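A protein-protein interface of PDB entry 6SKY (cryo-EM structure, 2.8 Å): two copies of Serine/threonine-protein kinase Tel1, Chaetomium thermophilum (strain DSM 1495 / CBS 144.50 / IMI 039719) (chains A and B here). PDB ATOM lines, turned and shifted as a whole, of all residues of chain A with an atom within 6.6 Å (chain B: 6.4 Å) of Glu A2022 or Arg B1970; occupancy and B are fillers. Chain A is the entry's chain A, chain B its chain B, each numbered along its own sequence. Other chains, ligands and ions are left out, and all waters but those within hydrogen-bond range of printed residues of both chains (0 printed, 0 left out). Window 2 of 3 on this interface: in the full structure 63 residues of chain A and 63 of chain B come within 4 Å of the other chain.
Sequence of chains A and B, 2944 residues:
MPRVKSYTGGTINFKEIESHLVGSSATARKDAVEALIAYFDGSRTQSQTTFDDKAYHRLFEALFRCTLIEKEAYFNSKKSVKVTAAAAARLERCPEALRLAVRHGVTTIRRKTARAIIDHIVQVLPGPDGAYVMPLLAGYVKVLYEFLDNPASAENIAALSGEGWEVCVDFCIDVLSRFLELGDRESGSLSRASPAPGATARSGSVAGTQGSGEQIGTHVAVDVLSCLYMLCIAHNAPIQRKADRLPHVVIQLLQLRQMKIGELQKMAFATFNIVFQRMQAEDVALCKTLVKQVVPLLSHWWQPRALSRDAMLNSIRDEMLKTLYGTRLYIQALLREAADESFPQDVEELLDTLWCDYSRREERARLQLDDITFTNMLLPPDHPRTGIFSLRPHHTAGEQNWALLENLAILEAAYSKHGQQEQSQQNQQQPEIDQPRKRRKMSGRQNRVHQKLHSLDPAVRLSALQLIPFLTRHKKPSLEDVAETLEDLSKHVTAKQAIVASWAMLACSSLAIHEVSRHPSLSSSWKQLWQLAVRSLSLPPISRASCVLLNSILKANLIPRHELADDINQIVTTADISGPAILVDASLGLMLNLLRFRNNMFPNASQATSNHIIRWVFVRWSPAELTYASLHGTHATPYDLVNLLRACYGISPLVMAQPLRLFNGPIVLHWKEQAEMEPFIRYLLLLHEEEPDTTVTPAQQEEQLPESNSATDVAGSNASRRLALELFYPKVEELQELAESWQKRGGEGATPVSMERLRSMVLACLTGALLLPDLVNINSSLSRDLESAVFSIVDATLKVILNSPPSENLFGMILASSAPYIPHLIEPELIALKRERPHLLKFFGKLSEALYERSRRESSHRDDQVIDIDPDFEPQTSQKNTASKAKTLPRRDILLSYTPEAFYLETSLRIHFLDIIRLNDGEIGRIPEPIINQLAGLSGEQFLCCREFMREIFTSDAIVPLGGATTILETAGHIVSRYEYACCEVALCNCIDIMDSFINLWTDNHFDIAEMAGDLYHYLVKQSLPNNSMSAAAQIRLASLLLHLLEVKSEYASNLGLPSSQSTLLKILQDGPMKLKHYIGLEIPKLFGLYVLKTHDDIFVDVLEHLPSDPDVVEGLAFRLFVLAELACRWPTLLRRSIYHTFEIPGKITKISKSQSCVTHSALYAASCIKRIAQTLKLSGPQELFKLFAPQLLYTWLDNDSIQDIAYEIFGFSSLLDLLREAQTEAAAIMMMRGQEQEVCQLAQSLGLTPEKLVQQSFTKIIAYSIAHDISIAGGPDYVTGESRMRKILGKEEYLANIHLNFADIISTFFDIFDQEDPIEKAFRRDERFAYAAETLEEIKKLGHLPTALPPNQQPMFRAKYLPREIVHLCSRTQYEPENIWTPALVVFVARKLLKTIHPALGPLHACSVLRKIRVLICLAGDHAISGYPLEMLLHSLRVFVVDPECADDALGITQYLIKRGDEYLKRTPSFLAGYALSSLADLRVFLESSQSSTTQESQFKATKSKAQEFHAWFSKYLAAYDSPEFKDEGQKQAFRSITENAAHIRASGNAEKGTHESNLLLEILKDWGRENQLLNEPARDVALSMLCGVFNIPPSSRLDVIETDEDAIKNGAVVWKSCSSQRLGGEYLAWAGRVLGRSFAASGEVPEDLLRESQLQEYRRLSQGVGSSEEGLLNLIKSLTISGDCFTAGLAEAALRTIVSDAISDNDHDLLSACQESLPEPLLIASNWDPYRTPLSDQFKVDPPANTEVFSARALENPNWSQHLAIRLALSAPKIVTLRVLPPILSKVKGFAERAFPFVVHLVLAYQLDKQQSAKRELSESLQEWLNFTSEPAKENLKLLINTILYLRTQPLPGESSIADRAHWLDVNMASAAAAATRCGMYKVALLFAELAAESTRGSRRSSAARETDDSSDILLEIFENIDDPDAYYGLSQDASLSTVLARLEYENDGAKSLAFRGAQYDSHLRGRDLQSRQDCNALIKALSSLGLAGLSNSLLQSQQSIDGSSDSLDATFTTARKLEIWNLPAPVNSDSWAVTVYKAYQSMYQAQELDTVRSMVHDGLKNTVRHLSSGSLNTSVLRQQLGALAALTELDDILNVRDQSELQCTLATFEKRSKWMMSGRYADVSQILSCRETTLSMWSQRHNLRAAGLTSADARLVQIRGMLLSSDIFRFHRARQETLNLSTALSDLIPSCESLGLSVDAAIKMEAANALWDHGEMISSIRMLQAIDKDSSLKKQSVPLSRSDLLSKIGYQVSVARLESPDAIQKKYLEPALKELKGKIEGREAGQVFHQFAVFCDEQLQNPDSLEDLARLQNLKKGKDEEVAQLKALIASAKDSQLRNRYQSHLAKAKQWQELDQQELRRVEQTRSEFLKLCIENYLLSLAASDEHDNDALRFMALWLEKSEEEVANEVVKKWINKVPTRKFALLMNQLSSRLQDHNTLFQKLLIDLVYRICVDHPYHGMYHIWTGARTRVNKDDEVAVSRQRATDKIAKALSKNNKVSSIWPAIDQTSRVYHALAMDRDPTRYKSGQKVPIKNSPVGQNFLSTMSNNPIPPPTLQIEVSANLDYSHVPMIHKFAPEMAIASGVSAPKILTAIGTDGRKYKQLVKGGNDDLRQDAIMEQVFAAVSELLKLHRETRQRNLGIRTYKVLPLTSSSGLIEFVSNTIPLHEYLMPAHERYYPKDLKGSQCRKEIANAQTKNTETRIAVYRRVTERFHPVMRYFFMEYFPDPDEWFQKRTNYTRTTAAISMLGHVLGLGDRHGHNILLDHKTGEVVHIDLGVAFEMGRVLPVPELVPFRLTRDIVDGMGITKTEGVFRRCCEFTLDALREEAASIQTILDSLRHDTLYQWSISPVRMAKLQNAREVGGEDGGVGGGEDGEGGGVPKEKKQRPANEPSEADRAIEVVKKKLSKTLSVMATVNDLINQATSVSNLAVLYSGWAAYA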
ATOM      1  N   THR A2017      16.176  -0.242  -5.803  1.00  0.00           N
ATOM      2  CA  THR A2017      15.171   0.643  -5.235  1.00  0.00           C
ATOM      3  C   THR A2017      13.768   0.121  -5.484  1.00  0.00           C
ATOM      4  O   THR A2017      12.904   0.205  -4.607  1.00  0.00           O
ATOM      5  CB  THR A2017      15.335   2.035  -5.824  1.00  0.00           C
ATOM      6  OG1 THR A2017      16.671   2.487  -5.601  1.00  0.00           O
ATOM      7  CG2 THR A2017      14.387   2.991  -5.183  1.00  0.00           C
ATOM      8  N   ALA A2018      13.520  -0.426  -6.672  1.00  0.00           N
ATOM      9  CA  ALA A2018      12.208  -0.982  -6.960  1.00  0.00           C
ATOM     10  C   ALA A2018      11.900  -2.170  -6.067  1.00  0.00           C
ATOM     11  O   ALA A2018      10.754  -2.358  -5.658  1.00  0.00           O
ATOM     12  CB  ALA A2018      12.125  -1.382  -8.425  1.00  0.00           C
ATOM     13  N   ARG A2019      12.905  -2.989  -5.756  1.00  0.00           N
ATOM     14  CA  ARG A2019      12.661  -4.128  -4.880  1.00  0.00           C
ATOM     15  C   ARG A2019      12.467  -3.697  -3.434  1.00  0.00           C
ATOM     16  O   ARG A2019      11.653  -4.280  -2.714  1.00  0.00           O
ATOM     17  CB  ARG A2019      13.806  -5.119  -4.985  1.00  0.00           C
ATOM     18  CG  ARG A2019      13.604  -6.340  -4.148  1.00  0.00           C
ATOM     19  CD  ARG A2019      14.795  -7.249  -4.189  1.00  0.00           C
ATOM     20  NE  ARG A2019      16.034  -6.572  -3.845  1.00  0.00           N
ATOM     21  CZ  ARG A2019      16.384  -6.243  -2.614  1.00  0.00           C
ATOM     22  NH1 ARG A2019      17.531  -5.632  -2.396  1.00  0.00           N
ATOM     23  NH2 ARG A2019      15.581  -6.505  -1.607  1.00  0.00           N
ATOM     24  N   LYS A2020      13.208  -2.687  -2.983  1.00  0.00           N
ATOM     25  CA  LYS A2020      13.065  -2.237  -1.604  1.00  0.00           C
ATOM     26  C   LYS A2020      11.731  -1.548  -1.372  1.00  0.00           C
ATOM     27  O   LYS A2020      11.106  -1.742  -0.328  1.00  0.00           O
ATOM     28  CB  LYS A2020      14.208  -1.306  -1.234  1.00  0.00           C
ATOM     29  CG  LYS A2020      15.505  -2.008  -1.007  1.00  0.00           C
ATOM     30  CD  LYS A2020      16.603  -1.012  -0.782  1.00  0.00           C
ATOM     31  CE  LYS A2020      17.906  -1.708  -0.503  1.00  0.00           C
ATOM     32  NZ  LYS A2020      17.767  -2.589   0.674  1.00  0.00           N
ATOM     33  N   LEU A2021      11.282  -0.726  -2.315  1.00  0.00           N
ATOM     34  CA  LEU A2021       9.984  -0.084  -2.167  1.00  0.00           C
ATOM     35  C   LEU A2021       8.832  -0.963  -2.618  1.00  0.00           C
ATOM     36  O   LEU A2021       7.678  -0.573  -2.438  1.00  0.00           O
ATOM     37  CB  LEU A2021       9.950   1.224  -2.947  1.00  0.00           C
ATOM     38  CG  LEU A2021      10.873   2.304  -2.407  1.00  0.00           C
ATOM     39  CD1 LEU A2021      10.889   3.485  -3.333  1.00  0.00           C
ATOM     40  CD2 LEU A2021      10.426   2.710  -1.034  1.00  0.00           C
ATOM     41  N   GLU A2022       9.120  -2.123  -3.203  1.00  0.00           N
ATOM     42  CA  GLU A2022       8.119  -3.068  -3.688  1.00  0.00           C
ATOM     43  C   GLU A2022       7.260  -2.459  -4.793  1.00  0.00           C
ATOM     44  O   GLU A2022       6.045  -2.343  -4.685  1.00  0.00           O
ATOM     45  CB  GLU A2022       7.266  -3.582  -2.537  1.00  0.00           C
ATOM     46  CG  GLU A2022       8.074  -4.334  -1.528  1.00  0.00           C
ATOM     47  CD  GLU A2022       7.218  -5.076  -0.549  1.00  0.00           C
ATOM     48  OE1 GLU A2022       6.016  -4.768  -0.474  1.00  0.00           O
ATOM     49  OE2 GLU A2022       7.742  -5.975   0.140  1.00  0.00           O
ATOM     50  N   ILE A2023       7.931  -2.082  -5.870  1.00  0.00           N
ATOM     51  CA  ILE A2023       7.312  -1.560  -7.079  1.00  0.00           C
ATOM     52  C   ILE A2023       7.477  -2.638  -8.136  1.00  0.00           C
ATOM     53  O   ILE A2023       8.515  -2.719  -8.795  1.00  0.00           O
ATOM     54  CB  ILE A2023       7.955  -0.246  -7.522  1.00  0.00           C
ATOM     55  CG1 ILE A2023       7.773   0.819  -6.454  1.00  0.00           C
ATOM     56  CG2 ILE A2023       7.385   0.211  -8.830  1.00  0.00           C
ATOM     57  CD1 ILE A2023       8.693   1.978  -6.627  1.00  0.00           C
ATOM     58  N   TRP A2024       6.462  -3.475  -8.306  1.00  0.00           N
ATOM     59  CA  TRP A2024       6.610  -4.709  -9.055  1.00  0.00           C
ATOM     60  C   TRP A2024       6.162  -4.596 -10.501  1.00  0.00           C
ATOM     61  O   TRP A2024       5.833  -5.612 -11.114  1.00  0.00           O
ATOM     62  CB  TRP A2024       5.844  -5.828  -8.364  1.00  0.00           C
ATOM     63  CG  TRP A2024       6.277  -6.117  -6.975  1.00  0.00           C
ATOM     64  CD1 TRP A2024       5.489  -6.170  -5.877  1.00  0.00           C
ATOM     65  CD2 TRP A2024       7.603  -6.410  -6.531  1.00  0.00           C
ATOM     66  NE1 TRP A2024       6.233  -6.473  -4.776  1.00  0.00           N
ATOM     67  CE2 TRP A2024       7.538  -6.625  -5.154  1.00  0.00           C
ATOM     68  CE3 TRP A2024       8.838  -6.505  -7.167  1.00  0.00           C
ATOM     69  CZ2 TRP A2024       8.653  -6.925  -4.405  1.00  0.00           C
ATOM     70  CZ3 TRP A2024       9.930  -6.803  -6.424  1.00  0.00           C
ATOM     71  CH2 TRP A2024       9.837  -7.013  -5.060  1.00  0.00           C
ATOM     72  N   ASN A2025       6.160  -3.399 -11.074  1.00  0.00           N
ATOM     73  CA  ASN A2025       5.678  -3.207 -12.434  1.00  0.00           C
ATOM     74  C   ASN A2025       6.730  -2.572 -13.330  1.00  0.00           C
ATOM     75  O   ASN A2025       6.396  -1.883 -14.288  1.00  0.00           O
ATOM     76  CB  ASN A2025       4.398  -2.376 -12.446  1.00  0.00           C
ATOM     77  CG  ASN A2025       4.579  -1.009 -11.834  1.00  0.00           C
ATOM     78  OD1 ASN A2025       5.485  -0.264 -12.193  1.00  0.00           O
ATOM     79  ND2 ASN A2025       3.708  -0.669 -10.901  1.00  0.00           N
ATOM     80  N   TYR A2040      15.192  -9.139  -8.902  1.00  0.00           N
ATOM     81  CA  TYR A2040      13.942  -8.430  -9.108  1.00  0.00           C
ATOM     82  C   TYR A2040      12.962  -9.253  -9.918  1.00  0.00           C
ATOM     83  O   TYR A2040      11.772  -9.273  -9.614  1.00  0.00           O
ATOM     84  CB  TYR A2040      14.207  -7.108  -9.809  1.00  0.00           C
ATOM     85  CG  TYR A2040      12.965  -6.297 -10.010  1.00  0.00           C
ATOM     86  CD1 TYR A2040      12.367  -5.661  -8.949  1.00  0.00           C
ATOM     87  CD2 TYR A2040      12.388  -6.170 -11.255  1.00  0.00           C
ATOM     88  CE1 TYR A2040      11.241  -4.932  -9.117  1.00  0.00           C
ATOM     89  CE2 TYR A2040      11.258  -5.437 -11.428  1.00  0.00           C
ATOM     90  CZ  TYR A2040      10.690  -4.820 -10.352  1.00  0.00           C
ATOM     91  OH  TYR A2040       9.558  -4.078 -10.506  1.00  0.00           O
ATOM     92  N   GLU A2135      14.851 -10.047   3.806  1.00  0.00           N
ATOM     93  CA  GLU A2135      13.705  -9.260   4.245  1.00  0.00           C
ATOM     94  C   GLU A2135      12.622  -9.212   3.178  1.00  0.00           C
ATOM     95  O   GLU A2135      11.432  -9.392   3.472  1.00  0.00           O
ATOM     96  CB  GLU A2135      14.168  -7.858   4.596  1.00  0.00           C
ATOM     97  CG  GLU A2135      13.095  -6.956   5.093  1.00  0.00           C
ATOM     98  CD  GLU A2135      13.426  -5.518   4.822  1.00  0.00           C
ATOM     99  OE1 GLU A2135      14.230  -5.271   3.901  1.00  0.00           O
ATOM    100  OE2 GLU A2135      12.894  -4.633   5.524  1.00  0.00           O
ATOM    101  N   THR A2136      13.017  -8.950   1.931  1.00  0.00           N
ATOM    102  CA  THR A2136      12.045  -8.953   0.838  1.00  0.00           C
ATOM    103  C   THR A2136      11.359 -10.305   0.704  1.00  0.00           C
ATOM    104  O   THR A2136      10.140 -10.377   0.524  1.00  0.00           O
ATOM    105  CB  THR A2136      12.717  -8.583  -0.474  1.00  0.00           C
ATOM    106  OG1 THR A2136      13.358  -7.318  -0.333  1.00  0.00           O
ATOM    107  CG2 THR A2136      11.702  -8.479  -1.556  1.00  0.00           C
ATOM    108  N   SER A2139       8.756 -10.833   3.607  1.00  0.00           N
ATOM    109  CA  SER A2139       7.555 -10.010   3.502  1.00  0.00           C
ATOM    110  C   SER A2139       6.680 -10.446   2.335  1.00  0.00           C
ATOM    111  O   SER A2139       5.454 -10.543   2.477  1.00  0.00           O
ATOM    112  CB  SER A2139       7.926  -8.541   3.370  1.00  0.00           C
ATOM    113  OG  SER A2139       8.270  -8.226   2.046  1.00  0.00           O
ATOM    114  N   MET A2140       7.284 -10.725   1.176  1.00  0.00           N
ATOM    115  CA  MET A2140       6.505 -11.196   0.037  1.00  0.00           C
ATOM    116  C   MET A2140       5.796 -12.501   0.349  1.00  0.00           C
ATOM    117  O   MET A2140       4.642 -12.693  -0.037  1.00  0.00           O
ATOM    118  CB  MET A2140       7.401 -11.369  -1.181  1.00  0.00           C
ATOM    119  CG  MET A2140       7.788 -10.085  -1.850  1.00  0.00           C
ATOM    120  SD  MET A2140       6.396  -9.287  -2.637  1.00  0.00           S
ATOM    121  CE  MET A2140       5.816 -10.623  -3.650  1.00  0.00           C
ATOM    122  N   GLN A2143       2.766 -11.869   2.369  1.00  0.00           N
ATOM    123  CA  GLN A2143       1.664 -11.200   1.684  1.00  0.00           C
ATOM    124  C   GLN A2143       0.897 -12.132   0.755  1.00  0.00           C
ATOM    125  O   GLN A2143      -0.326 -12.024   0.642  1.00  0.00           O
ATOM    126  CB  GLN A2143       2.185 -10.014   0.885  1.00  0.00           C
ATOM    127  CG  GLN A2143       2.695  -8.882   1.723  1.00  0.00           C
ATOM    128  CD  GLN A2143       3.301  -7.797   0.886  1.00  0.00           C
ATOM    129  OE1 GLN A2143       3.299  -7.870  -0.338  1.00  0.00           O
ATOM    130  NE2 GLN A2143       3.834  -6.779   1.538  1.00  0.00           N
ATOM    131  N   SER B1965       9.272   3.528   4.768  1.00  0.00           N
ATOM    132  CA  SER B1965       8.294   2.602   5.313  1.00  0.00           C
ATOM    133  C   SER B1965       6.879   2.959   4.891  1.00  0.00           C
ATOM    134  O   SER B1965       6.013   2.083   4.831  1.00  0.00           O
ATOM    135  CB  SER B1965       8.403   2.571   6.827  1.00  0.00           C
ATOM    136  OG  SER B1965       7.278   1.937   7.377  1.00  0.00           O
ATOM    137  N   HIS B1966       6.618   4.233   4.604  1.00  0.00           N
ATOM    138  CA  HIS B1966       5.286   4.640   4.178  1.00  0.00           C
ATOM    139  C   HIS B1966       5.073   4.510   2.682  1.00  0.00           C
ATOM    140  O   HIS B1966       3.947   4.269   2.252  1.00  0.00           O
ATOM    141  CB  HIS B1966       5.006   6.076   4.607  1.00  0.00           C
ATOM    142  CG  HIS B1966       4.629   6.206   6.044  1.00  0.00           C
ATOM    143  ND1 HIS B1966       4.878   7.341   6.780  1.00  0.00           N
ATOM    144  CD2 HIS B1966       4.022   5.339   6.885  1.00  0.00           C
ATOM    145  CE1 HIS B1966       4.443   7.168   8.013  1.00  0.00           C
ATOM    146  NE2 HIS B1966       3.920   5.961   8.103  1.00  0.00           N
ATOM    147  N   LEU B1967       6.119   4.668   1.876  1.00  0.00           N
ATOM    148  CA  LEU B1967       5.992   4.372   0.455  1.00  0.00           C
ATOM    149  C   LEU B1967       5.810   2.882   0.219  1.00  0.00           C
ATOM    150  O   LEU B1967       5.019   2.477  -0.633  1.00  0.00           O
ATOM    151  CB  LEU B1967       7.217   4.857  -0.306  1.00  0.00           C
ATOM    152  CG  LEU B1967       7.466   6.339  -0.485  1.00  0.00           C
ATOM    153  CD1 LEU B1967       8.772   6.517  -1.205  1.00  0.00           C
ATOM    154  CD2 LEU B1967       6.345   6.945  -1.269  1.00  0.00           C
ATOM    155  N   ARG B1968       6.543   2.050   0.954  1.00  0.00           N
ATOM    156  CA  ARG B1968       6.461   0.613   0.732  1.00  0.00           C
ATOM    157  C   ARG B1968       5.100   0.064   1.131  1.00  0.00           C
ATOM    158  O   ARG B1968       4.542  -0.788   0.436  1.00  0.00           O
ATOM    159  CB  ARG B1968       7.569  -0.096   1.497  1.00  0.00           C
ATOM    160  CG  ARG B1968       7.397  -1.587   1.575  1.00  0.00           C
ATOM    161  CD  ARG B1968       8.619  -2.249   2.145  1.00  0.00           C
ATOM    162  NE  ARG B1968       8.925  -1.769   3.484  1.00  0.00           N
ATOM    163  CZ  ARG B1968       9.913  -0.930   3.772  1.00  0.00           C
ATOM    164  NH1 ARG B1968      10.703  -0.475   2.813  1.00  0.00           N
ATOM    165  NH2 ARG B1968      10.111  -0.550   5.022  1.00  0.00           N
ATOM    166  N   GLY B1969       4.553   0.534   2.235  1.00  0.00           N
ATOM    167  CA  GLY B1969       3.259   0.083   2.684  1.00  0.00           C
ATOM    168  C   GLY B1969       2.085   0.791   2.065  1.00  0.00           C
ATOM    169  O   GLY B1969       0.953   0.580   2.502  1.00  0.00           O
ATOM    170  N   ARG B1970       2.324   1.620   1.048  1.00  0.00           N
ATOM    171  CA  ARG B1970       1.278   2.388   0.380  1.00  0.00           C
ATOM    172  C   ARG B1970       0.449   3.175   1.386  1.00  0.00           C
ATOM    173  O   ARG B1970      -0.773   3.278   1.278  1.00  0.00           O
ATOM    174  CB  ARG B1970       0.391   1.488  -0.471  1.00  0.00           C
ATOM    175  CG  ARG B1970       0.839   1.378  -1.905  1.00  0.00           C
ATOM    176  CD  ARG B1970       2.025   0.475  -2.034  1.00  0.00           C
ATOM    177  NE  ARG B1970       2.591   0.527  -3.372  1.00  0.00           N
ATOM    178  CZ  ARG B1970       3.752  -0.017  -3.707  1.00  0.00           C
ATOM    179  NH1 ARG B1970       4.469  -0.655  -2.798  1.00  0.00           N
ATOM    180  NH2 ARG B1970       4.194   0.082  -4.949  1.00  0.00           N
ATOM    181  N   ASP B1971       1.123   3.728   2.382  1.00  0.00           N
ATOM    182  CA  ASP B1971       0.460   4.539   3.384  1.00  0.00           C
ATOM    183  C   ASP B1971       0.245   5.947   2.851  1.00  0.00           C
ATOM    184  O   ASP B1971       0.973   6.425   1.977  1.00  0.00           O
ATOM    185  CB  ASP B1971       1.286   4.566   4.667  1.00  0.00           C
ATOM    186  CG  ASP B1971       0.491   5.013   5.867  1.00  0.00           C
ATOM    187  OD1 ASP B1971      -0.277   5.988   5.751  1.00  0.00           O
ATOM    188  OD2 ASP B1971       0.633   4.390   6.936  1.00  0.00           O
ATOM    189  N   LEU B1972      -0.779   6.611   3.378  1.00  0.00           N
ATOM    190  CA  LEU B1972      -1.116   7.954   2.935  1.00  0.00           C
ATOM    191  C   LEU B1972      -0.316   9.033   3.642  1.00  0.00           C
ATOM    192  O   LEU B1972      -0.356  10.188   3.212  1.00  0.00           O
ATOM    193  CB  LEU B1972      -2.607   8.214   3.139  1.00  0.00           C
ATOM    194  CG  LEU B1972      -3.556   7.417   2.250  1.00  0.00           C
ATOM    195  CD1 LEU B1972      -4.986   7.694   2.655  1.00  0.00           C
ATOM    196  CD2 LEU B1972      -3.329   7.763   0.787  1.00  0.00           C
ATOM    197  N   SER B1974       2.870   9.247   3.651  1.00  0.00           N
ATOM    198  CA  SER B1974       4.116   9.510   2.941  1.00  0.00           C
ATOM    199  C   SER B1974       4.140  10.920   2.381  1.00  0.00           C
ATOM    200  O   SER B1974       5.185  11.578   2.387  1.00  0.00           O
ATOM    201  CB  SER B1974       4.320   8.483   1.834  1.00  0.00           C
ATOM    202  OG  SER B1974       3.100   8.166   1.198  1.00  0.00           O
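NH1 of Arg B1968 is in hydrogen-bond range of O of Lys A2020, at 3.4 Å. O of Leu A2021 is in hydrogen-bond range of NH1 of Arg B1970 (3.2 Å). The guanidinium group (NH1) of Arg B1970 sits at hydrogen-bond distance from the backbone carbonyl oxygen (O) of Glu A2022 (3.0 Å).
No position is printed for both chains. Of the 6 pairs that touch across the chains among the printed residues, none has its exchanged pair printed and touching as well.
Leu B1967 touches Leu A2021. Leu A2021 touches Arg B1968 (O to CA, 3.6 Å). Arg B1970 touches Ile A2023 (NH2 to CG1, 3.95 Å).
Of the printed residues of chain B, Lys A2020 touches Arg B1968 (3.4 Å). Of the printed residues of chain B, Leu A2021 touches Leu B1967 (3.9 Å), Arg B1968 (3.6 Å) and Arg B1970 (3.2 Å). Of the printed residues of chain B, Ile A2023 touches Arg B1970. Of the printed residues of chain A, Arg B1968 touches Lys A2020 (3.4 Å) and Leu A2021 (3.6 Å). Arg B1970 touches just these residues of chain A: Leu A2021 (3.2 Å), Glu A2022 (3.0 Å) and Ile A2023 (3.95 Å). Ser B1974 touches none of the printed residues of chain A. The nearest residue of chain B that does not touch Glu A2022 is Arg B1968 (4.03 Å). The nearest printed residue of chain A that does not touch Arg B1968 is Glu A2022 (4.03 Å).
The backbone carbonyl oxygen (O) of Ala A2018 is in hydrogen-bond range of the backbone NH (N) of Ile A2023 (2.8 Å). The side-chain carboxylate of Glu A2022 lies within hydrogen-bond range of the side-chain hydroxyl of Ser A2139, 3.0 Å away. The backbone carbonyl oxygen (O) of Ile A2023 lies within hydrogen-bond range of the side-chain hydroxyl (OH) of Tyr A2040 (2.4 Å). NH1 of Arg B1970 lies within hydrogen-bond range of O of Arg B1968, 3.2 Å away.
Of the 9 printed residues of chain B, 3 touch a printed residue of chain A. Printed residues of chain B that touch a printed residue of chain A: Leu B1967, Arg B1968 and Arg B1970. Among the printed residues, 6 pairs touch across the chains.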
